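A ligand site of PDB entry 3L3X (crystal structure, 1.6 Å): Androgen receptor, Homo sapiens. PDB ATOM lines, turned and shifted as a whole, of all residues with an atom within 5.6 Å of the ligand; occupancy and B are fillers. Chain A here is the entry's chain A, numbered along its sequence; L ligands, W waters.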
ATOM      1  N   LEU A  33      31.063 -17.486   8.904  1.00  0.00           N
ATOM      2  CA  LEU A  33      29.880 -17.604   8.033  1.00  0.00           C
ATOM      3  C   LEU A  33      29.397 -19.028   7.908  1.00  0.00           C
ATOM      4  O   LEU A  33      28.185 -19.258   7.889  1.00  0.00           O
ATOM      5  CB  LEU A  33      30.081 -16.946   6.675  1.00  0.00           C
ATOM      6  CG  LEU A  33      29.737 -15.452   6.618  1.00  0.00           C
ATOM      7  CD1 LEU A  33      28.239 -15.258   6.752  1.00  0.00           C
ATOM      8  CD2 LEU A  33      30.481 -14.679   7.659  1.00  0.00           C
ATOM      9  N   LEU A  36      27.366 -19.503  11.005  1.00  0.00           N
ATOM     10  CA  LEU A  36      26.078 -18.797  10.924  1.00  0.00           C
ATOM     11  C   LEU A  36      25.132 -19.569  10.014  1.00  0.00           C
ATOM     12  O   LEU A  36      23.958 -19.693  10.306  1.00  0.00           O
ATOM     13  CB  LEU A  36      26.261 -17.374  10.417  1.00  0.00           C
ATOM     14  CG  LEU A  36      26.769 -16.355  11.415  1.00  0.00           C
ATOM     15  CD1 LEU A  36      27.117 -15.041  10.687  1.00  0.00           C
ATOM     16  CD2 LEU A  36      25.712 -16.101  12.491  1.00  0.00           C
ATOM     17  N   ASN A  37      25.635 -20.122   8.913  1.00  0.00           N
ATOM     18  CA  ASN A  37      24.809 -20.931   8.014  1.00  0.00           C
ATOM     19  C   ASN A  37      24.269 -22.201   8.694  1.00  0.00           C
ATOM     20  O   ASN A  37      23.101 -22.571   8.512  1.00  0.00           O
ATOM     21  CB  ASN A  37      25.560 -21.301   6.738  1.00  0.00           C
ATOM     22  CG  ASN A  37      25.788 -20.129   5.818  1.00  0.00           C
ATOM     23  OD1 ASN A  37      25.060 -19.115   5.892  1.00  0.00           O
ATOM     24  ND2 ASN A  37      26.749 -20.285   4.885  1.00  0.00           N
ATOM     25  N   LEU A  39      23.838 -22.501  11.940  1.00  0.00           N
ATOM     26  CA  LEU A  39      22.844 -21.984  12.890  1.00  0.00           C
ATOM     27  C   LEU A  39      21.506 -21.722  12.208  1.00  0.00           C
ATOM     28  O   LEU A  39      20.444 -22.024  12.757  1.00  0.00           O
ATOM     29  CB  LEU A  39      23.339 -20.713  13.566  1.00  0.00           C
ATOM     30  CG  LEU A  39      22.387 -20.107  14.599  1.00  0.00           C
ATOM     31  CD1 LEU A  39      22.147 -21.105  15.752  1.00  0.00           C
ATOM     32  CD2 LEU A  39      22.961 -18.805  15.140  1.00  0.00           C
ATOM     33  N   GLY A  40      21.547 -21.153  11.005  1.00  0.00           N
ATOM     34  CA  GLY A  40      20.354 -20.966  10.212  1.00  0.00           C
ATOM     35  C   GLY A  40      19.615 -22.249   9.937  1.00  0.00           C
ATOM     36  O   GLY A  40      18.406 -22.336  10.078  1.00  0.00           O
ATOM     37  N   GLN A  43      18.088 -23.438  13.248  1.00  0.00           N
ATOM     38  CA  GLN A  43      16.956 -22.627  13.607  1.00  0.00           C
ATOM     39  C   GLN A  43      15.745 -22.864  12.679  1.00  0.00           C
ATOM     40  O   GLN A  43      14.606 -22.756  13.110  1.00  0.00           O
ATOM     41  CB  GLN A  43      17.308 -21.144  13.692  1.00  0.00           C
ATOM     42  CG  GLN A  43      18.171 -20.795  14.908  1.00  0.00           C
ATOM     43  CD  GLN A  43      18.276 -19.329  15.132  1.00  0.00           C
ATOM     44  OE1 GLN A  43      17.550 -18.565  14.519  1.00  0.00           O
ATOM     45  NE2 GLN A  43      19.218 -18.908  15.980  1.00  0.00           N
ATOM     46  N   TRP A  73      11.637 -16.428   7.217  1.00  0.00           N
ATOM     47  CA  TRP A  73      12.608 -16.926   8.206  1.00  0.00           C
ATOM     48  C   TRP A  73      13.682 -15.905   8.578  1.00  0.00           C
ATOM     49  O   TRP A  73      14.038 -15.810   9.753  1.00  0.00           O
ATOM     50  CB  TRP A  73      13.268 -18.233   7.785  1.00  0.00           C
ATOM     51  CG  TRP A  73      14.034 -18.170   6.526  1.00  0.00           C
ATOM     52  CD1 TRP A  73      13.549 -18.409   5.301  1.00  0.00           C
ATOM     53  CD2 TRP A  73      15.435 -17.870   6.352  1.00  0.00           C
ATOM     54  NE1 TRP A  73      14.530 -18.267   4.357  1.00  0.00           N
ATOM     55  CE2 TRP A  73      15.704 -17.943   4.980  1.00  0.00           C
ATOM     56  CE3 TRP A  73      16.473 -17.547   7.228  1.00  0.00           C
ATOM     57  CZ2 TRP A  73      16.977 -17.718   4.443  1.00  0.00           C
ATOM     58  CZ3 TRP A  73      17.741 -17.332   6.708  1.00  0.00           C
ATOM     59  CH2 TRP A  73      17.982 -17.407   5.323  1.00  0.00           C
ATOM     60  N   MET A  74      14.212 -15.175   7.599  1.00  0.00           N
ATOM     61  CA  MET A  74      15.283 -14.222   7.917  1.00  0.00           C
ATOM     62  C   MET A  74      14.805 -13.168   8.921  1.00  0.00           C
ATOM     63  O   MET A  74      15.444 -12.926   9.949  1.00  0.00           O
ATOM     64  CB  MET A  74      15.816 -13.549   6.648  1.00  0.00           C
ATOM     65  CG  MET A  74      16.956 -12.621   6.918  1.00  0.00           C
ATOM     66  SD  MET A  74      18.516 -13.416   7.198  1.00  0.00           S
ATOM     67  CE  MET A  74      18.939 -13.818   5.506  1.00  0.00           C
ATOM     68  N   MET A  77      14.168 -14.743  12.421  1.00  0.00           N
ATOM     69  CA  MET A  77      15.397 -15.106  13.124  1.00  0.00           C
ATOM     70  C   MET A  77      16.158 -13.880  13.583  1.00  0.00           C
ATOM     71  O   MET A  77      16.743 -13.873  14.684  1.00  0.00           O
ATOM     72  CB  MET A  77      16.267 -15.978  12.259  1.00  0.00           C
ATOM     73  CG  MET A  77      15.744 -17.397  12.072  1.00  0.00           C
ATOM     74  SD  MET A  77      16.853 -18.329  11.006  1.00  0.00           S
ATOM     75  CE  MET A  77      15.814 -19.759  10.674  1.00  0.00           C
ATOM     76  N   VAL A  78      16.197 -12.853  12.748  1.00  0.00           N
ATOM     77  CA  VAL A  78      16.846 -11.566  13.151  1.00  0.00           C
ATOM     78  C   VAL A  78      16.147 -10.912  14.321  1.00  0.00           C
ATOM     79  O   VAL A  78      16.801 -10.453  15.264  1.00  0.00           O
ATOM     80  CB  VAL A  78      16.957 -10.621  11.977  1.00  0.00           C
ATOM     81  CG1 VAL A  78      17.411  -9.205  12.417  1.00  0.00           C
ATOM     82  CG2 VAL A  78      17.945 -11.210  10.932  1.00  0.00           C
ATOM     83  N   MET A  81      16.886 -12.864  17.409  1.00  0.00           N
ATOM     84  CA  MET A  81      18.283 -12.625  17.774  1.00  0.00           C
ATOM     85  C   MET A  81      18.428 -11.268  18.451  1.00  0.00           C
ATOM     86  O   MET A  81      19.143 -11.153  19.458  1.00  0.00           O
ATOM     87  CB  MET A  81      19.195 -12.776  16.555  1.00  0.00           C
ATOM     88  CG  MET A  81      20.681 -12.748  16.891  1.00  0.00           C
ATOM     89  SD  MET A  81      21.317 -11.092  16.992  1.00  0.00           S
ATOM     90  CE  MET A  81      21.164 -10.532  15.316  1.00  0.00           C
ATOM     91  N   ARG A  84      17.277 -11.695  22.029  1.00  0.00           N
ATOM     92  CA  ARG A  84      18.292 -12.422  22.825  1.00  0.00           C
ATOM     93  C   ARG A  84      19.444 -11.502  23.168  1.00  0.00           C
ATOM     94  O   ARG A  84      20.001 -11.588  24.252  1.00  0.00           O
ATOM     95  CB  ARG A  84      18.871 -13.606  22.041  1.00  0.00           C
ATOM     96  CG  ARG A  84      17.929 -14.762  21.823  1.00  0.00           C
ATOM     97  CD  ARG A  84      18.684 -16.015  21.447  1.00  0.00           C
ATOM     98  NE  ARG A  84      19.311 -15.943  20.127  1.00  0.00           N
ATOM     99  CZ  ARG A  84      18.650 -16.065  18.977  1.00  0.00           C
ATOM    100  NH1 ARG A  84      17.330 -16.203  18.935  1.00  0.00           N
ATOM    101  NH2 ARG A  84      19.331 -16.029  17.841  1.00  0.00           N
ATOM    102  N   TYR A  95      24.015 -11.722  20.030  1.00  0.00           N
ATOM    103  CA  TYR A  95      23.907 -13.043  20.615  1.00  0.00           C
ATOM    104  C   TYR A  95      23.218 -13.978  19.634  1.00  0.00           C
ATOM    105  O   TYR A  95      22.042 -14.335  19.787  1.00  0.00           O
ATOM    106  CB  TYR A  95      23.147 -12.944  21.948  1.00  0.00           C
ATOM    107  CG  TYR A  95      23.357 -14.107  22.896  1.00  0.00           C
ATOM    108  CD1 TYR A  95      22.702 -15.315  22.710  1.00  0.00           C
ATOM    109  CD2 TYR A  95      24.220 -14.001  23.992  1.00  0.00           C
ATOM    110  CE1 TYR A  95      22.861 -16.376  23.601  1.00  0.00           C
ATOM    111  CE2 TYR A  95      24.402 -15.064  24.879  1.00  0.00           C
ATOM    112  CZ  TYR A  95      23.716 -16.229  24.682  1.00  0.00           C
ATOM    113  OH  TYR A  95      23.902 -17.287  25.560  1.00  0.00           O
ATOM    114  N   PHE A  96      23.953 -14.386  18.599  1.00  0.00           N
ATOM    115  CA  PHE A  96      23.375 -15.345  17.646  1.00  0.00           C
ATOM    116  C   PHE A  96      23.024 -16.650  18.330  1.00  0.00           C
ATOM    117  O   PHE A  96      21.966 -17.224  18.093  1.00  0.00           O
ATOM    118  CB  PHE A  96      24.336 -15.577  16.484  1.00  0.00           C
ATOM    119  CG  PHE A  96      24.514 -14.392  15.601  1.00  0.00           C
ATOM    120  CD1 PHE A  96      23.504 -14.029  14.702  1.00  0.00           C
ATOM    121  CD2 PHE A  96      25.708 -13.687  15.576  1.00  0.00           C
ATOM    122  CE1 PHE A  96      23.667 -12.932  13.872  1.00  0.00           C
ATOM    123  CE2 PHE A  96      25.846 -12.601  14.754  1.00  0.00           C
ATOM    124  CZ  PHE A  96      24.847 -12.223  13.904  1.00  0.00           C
ATOM    125  N   MET A 112      30.265  -8.384   7.276  1.00  0.00           N
ATOM    126  CA  MET A 112      28.937  -7.777   7.305  1.00  0.00           C
ATOM    127  C   MET A 112      28.794  -6.846   8.500  1.00  0.00           C
ATOM    128  O   MET A 112      27.786  -6.811   9.172  1.00  0.00           O
ATOM    129  CB  MET A 112      27.782  -8.806   7.190  1.00  0.00           C
ATOM    130  CG  MET A 112      27.902 -10.028   8.032  1.00  0.00           C
ATOM    131  SD  MET A 112      26.409 -11.068   7.865  1.00  0.00           S
ATOM    132  CE  MET A 112      25.605 -10.678   9.403  1.00  0.00           C
ATOM    133  N   MET A 119      21.561  -4.530  12.914  1.00  0.00           N
ATOM    134  CA  MET A 119      20.986  -5.521  13.831  1.00  0.00           C
ATOM    135  C   MET A 119      21.130  -5.119  15.289  1.00  0.00           C
ATOM    136  O   MET A 119      20.231  -5.343  16.095  1.00  0.00           O
ATOM    137  CB  MET A 119      21.566  -6.900  13.581  1.00  0.00           C
ATOM    138  CG  MET A 119      21.104  -7.514  12.266  1.00  0.00           C
ATOM    139  SD  MET A 119      21.503  -9.244  12.008  1.00  0.00           S
ATOM    140  CE  MET A 119      23.234  -9.134  11.482  1.00  0.00           C
ATOM    141  N   LEU A 205      20.391  -8.625   4.369  1.00  0.00           N
ATOM    142  CA  LEU A 205      20.910  -9.957   4.638  1.00  0.00           C
ATOM    143  C   LEU A 205      20.556 -10.961   3.538  1.00  0.00           C
ATOM    144  O   LEU A 205      21.395 -11.819   3.208  1.00  0.00           O
ATOM    145  CB  LEU A 205      20.483 -10.445   5.997  1.00  0.00           C
ATOM    146  CG  LEU A 205      20.970  -9.599   7.203  1.00  0.00           C
ATOM    147  CD1 LEU A 205      20.217 -10.002   8.461  1.00  0.00           C
ATOM    148  CD2 LEU A 205      22.462  -9.740   7.391  1.00  0.00           C
ATOM    149  N   PHE A 208      23.086 -10.207   0.885  1.00  0.00           N
ATOM    150  CA  PHE A 208      24.382 -10.725   1.302  1.00  0.00           C
ATOM    151  C   PHE A 208      24.499 -12.227   1.179  1.00  0.00           C
ATOM    152  O   PHE A 208      25.479 -12.742   0.629  1.00  0.00           O
ATOM    153  CB  PHE A 208      24.690 -10.280   2.727  1.00  0.00           C
ATOM    154  CG  PHE A 208      26.083 -10.598   3.201  1.00  0.00           C
ATOM    155  CD1 PHE A 208      26.361 -11.772   3.850  1.00  0.00           C
ATOM    156  CD2 PHE A 208      27.110  -9.671   3.034  1.00  0.00           C
ATOM    157  CE1 PHE A 208      27.667 -12.068   4.316  1.00  0.00           C
ATOM    158  CE2 PHE A 208      28.411  -9.950   3.483  1.00  0.00           C
ATOM    159  CZ  PHE A 208      28.675 -11.157   4.145  1.00  0.00           C
ATOM    160  N   THR A 209      23.522 -12.953   1.706  1.00  0.00           N
ATOM    161  CA  THR A 209      23.580 -14.416   1.682  1.00  0.00           C
ATOM    162  C   THR A 209      23.494 -14.974   0.251  1.00  0.00           C
ATOM    163  O   THR A 209      24.127 -15.938  -0.063  1.00  0.00           O
ATOM    164  CB  THR A 209      22.553 -15.054   2.646  1.00  0.00           C
ATOM    165  OG1 THR A 209      22.939 -16.395   2.943  1.00  0.00           O
ATOM    166  CG2 THR A 209      21.102 -15.001   2.089  1.00  0.00           C
ATOM    167  N   LEU A 212      26.785 -14.461  -1.269  1.00  0.00           N
ATOM    168  CA  LEU A 212      27.686 -15.424  -0.632  1.00  0.00           C
ATOM    169  C   LEU A 212      27.528 -16.827  -1.170  1.00  0.00           C
ATOM    170  O   LEU A 212      28.496 -17.515  -1.386  1.00  0.00           O
ATOM    171  CB  LEU A 212      27.508 -15.419   0.871  1.00  0.00           C
ATOM    172  CG  LEU A 212      28.464 -16.286   1.683  1.00  0.00           C
ATOM    173  CD1 LEU A 212      29.930 -15.989   1.386  1.00  0.00           C
ATOM    174  CD2 LEU A 212      28.187 -16.085   3.166  1.00  0.00           C
ATOM    175  N   PHE A 223      27.326 -24.110   2.902  1.00  0.00           N
ATOM    176  CA  PHE A 223      25.885 -23.905   3.101  1.00  0.00           C
ATOM    177  C   PHE A 223      25.217 -25.263   3.250  1.00  0.00           C
ATOM    178  O   PHE A 223      25.351 -26.133   2.358  1.00  0.00           O
ATOM    179  CB  PHE A 223      25.245 -23.212   1.917  1.00  0.00           C
ATOM    180  CG  PHE A 223      25.459 -21.720   1.891  1.00  0.00           C
ATOM    181  CD1 PHE A 223      26.669 -21.183   1.478  1.00  0.00           C
ATOM    182  CD2 PHE A 223      24.416 -20.865   2.214  1.00  0.00           C
ATOM    183  CE1 PHE A 223      26.837 -19.799   1.432  1.00  0.00           C
ATOM    184  CE2 PHE A 223      24.600 -19.457   2.177  1.00  0.00           C
ATOM    185  CZ  PHE A 223      25.799 -18.948   1.792  1.00  0.00           C
ATOM    186  N   MET A 227      19.229 -24.477   3.698  1.00  0.00           N
ATOM    187  CA  MET A 227      19.656 -23.098   3.419  1.00  0.00           C
ATOM    188  C   MET A 227      19.987 -22.872   1.941  1.00  0.00           C
ATOM    189  O   MET A 227      19.533 -21.887   1.332  1.00  0.00           O
ATOM    190  CB  MET A 227      20.881 -22.712   4.283  1.00  0.00           C
ATOM    191  CG  MET A 227      20.602 -22.605   5.770  1.00  0.00           C
ATOM    192  SD  MET A 227      19.615 -21.137   6.220  1.00  0.00           S
ATOM    193  CE  MET A 227      20.837 -19.827   6.172  1.00  0.00           C
HETATM  194  C1  LIG L   1      21.075 -17.202  11.817  1.00  0.00           C
HETATM  195  C2  LIG L   1      20.110 -17.168  13.007  1.00  0.00           C
HETATM  196  C3  LIG L   1      20.206 -15.848  13.728  1.00  0.00           C
HETATM  197  O1  LIG L   1      20.251 -15.825  14.949  1.00  0.00           O
HETATM  198  C4  LIG L   1      20.198 -14.610  12.878  1.00  0.00           C
HETATM  199  C5  LIG L   1      21.195 -14.749  11.712  1.00  0.00           C
HETATM  200  C6  LIG L   1      21.226 -13.440  10.883  1.00  0.00           C
HETATM  201  C7  LIG L   1      22.307 -13.516   9.811  1.00  0.00           C
HETATM  202  C8  LIG L   1      22.181 -14.767   8.922  1.00  0.00           C
HETATM  203  C9  LIG L   1      22.100 -16.050   9.784  1.00  0.00           C
HETATM  204  C10 LIG L   1      20.981 -16.004  10.873  1.00  0.00           C
HETATM  205  C11 LIG L   1      22.018 -17.323   8.899  1.00  0.00           C
HETATM  206  C12 LIG L   1      23.096 -17.391   7.807  1.00  0.00           C
HETATM  207  C13 LIG L   1      23.218 -16.086   6.998  1.00  0.00           C
HETATM  208  C14 LIG L   1      23.336 -14.899   7.943  1.00  0.00           C
HETATM  209  C15 LIG L   1      23.670 -13.735   7.011  1.00  0.00           C
HETATM  210  C16 LIG L   1      24.617 -14.359   5.966  1.00  0.00           C
HETATM  211  C17 LIG L   1      24.521 -15.867   6.199  1.00  0.00           C
HETATM  212  O2  LIG L   1      24.606 -16.628   4.972  1.00  0.00           O
HETATM  213  C18 LIG L   1      21.992 -15.974   6.098  1.00  0.00           C
HETATM  214  C19 LIG L   1      19.595 -16.022  10.214  1.00  0.00           C
HETATM  215  O   HOH W   1      17.133 -16.215  15.983  1.00  0.00           O
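The side-chain hydroxyl (OG1) of Thr 209 sits at hydrogen-bond distance from an oxygen (O2) of the ligand (2.6 Å). The side-chain amide oxygen (OD1) of Asn 37 is in hydrogen-bond range of an oxygen (O2) of the ligand (2.7 Å). O1 of the ligand lies within hydrogen-bond range of NH2 of Arg 84, 3.0 Å away. The side-chain amide nitrogen (NE2) of Gln 43 lies within hydrogen-bond range of an oxygen (O1) of the ligand (3.4 Å).
ND2 of Asn 37 sits close to O of Leu 33, 3.5 Å away. The side-chain amide nitrogen of Gln 43 lies close to the guanidinium group of Arg 84 (3.4 Å). The backbone carbonyl oxygen of Phe 96 lies within hydrogen-bond range of the guanidinium group of Arg 84. The guanidinium group (NE) of Arg 84 sits at hydrogen-bond distance from the backbone carbonyl oxygen (O) of Tyr 95 (3.2 Å). The side-chain amide oxygen (OE1) of Gln 43 sits close to the side-chain sulfur (SD) of Met 77.
Merely in contact with the ligand: Leu 33 (3.8 Å), Leu 36 (3.4 Å), Leu 39 (3.9 Å), Met 74 (3.8 Å), Met 77 (3.7 Å), Val 78 (3.97 Å), Met 81 (3.6 Å), Phe 96 (3.7 Å), Met 112 (3.9 Å), Phe 208 (3.8 Å), Phe 223 (3.98 Å) and Met 227 (3.7 Å).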
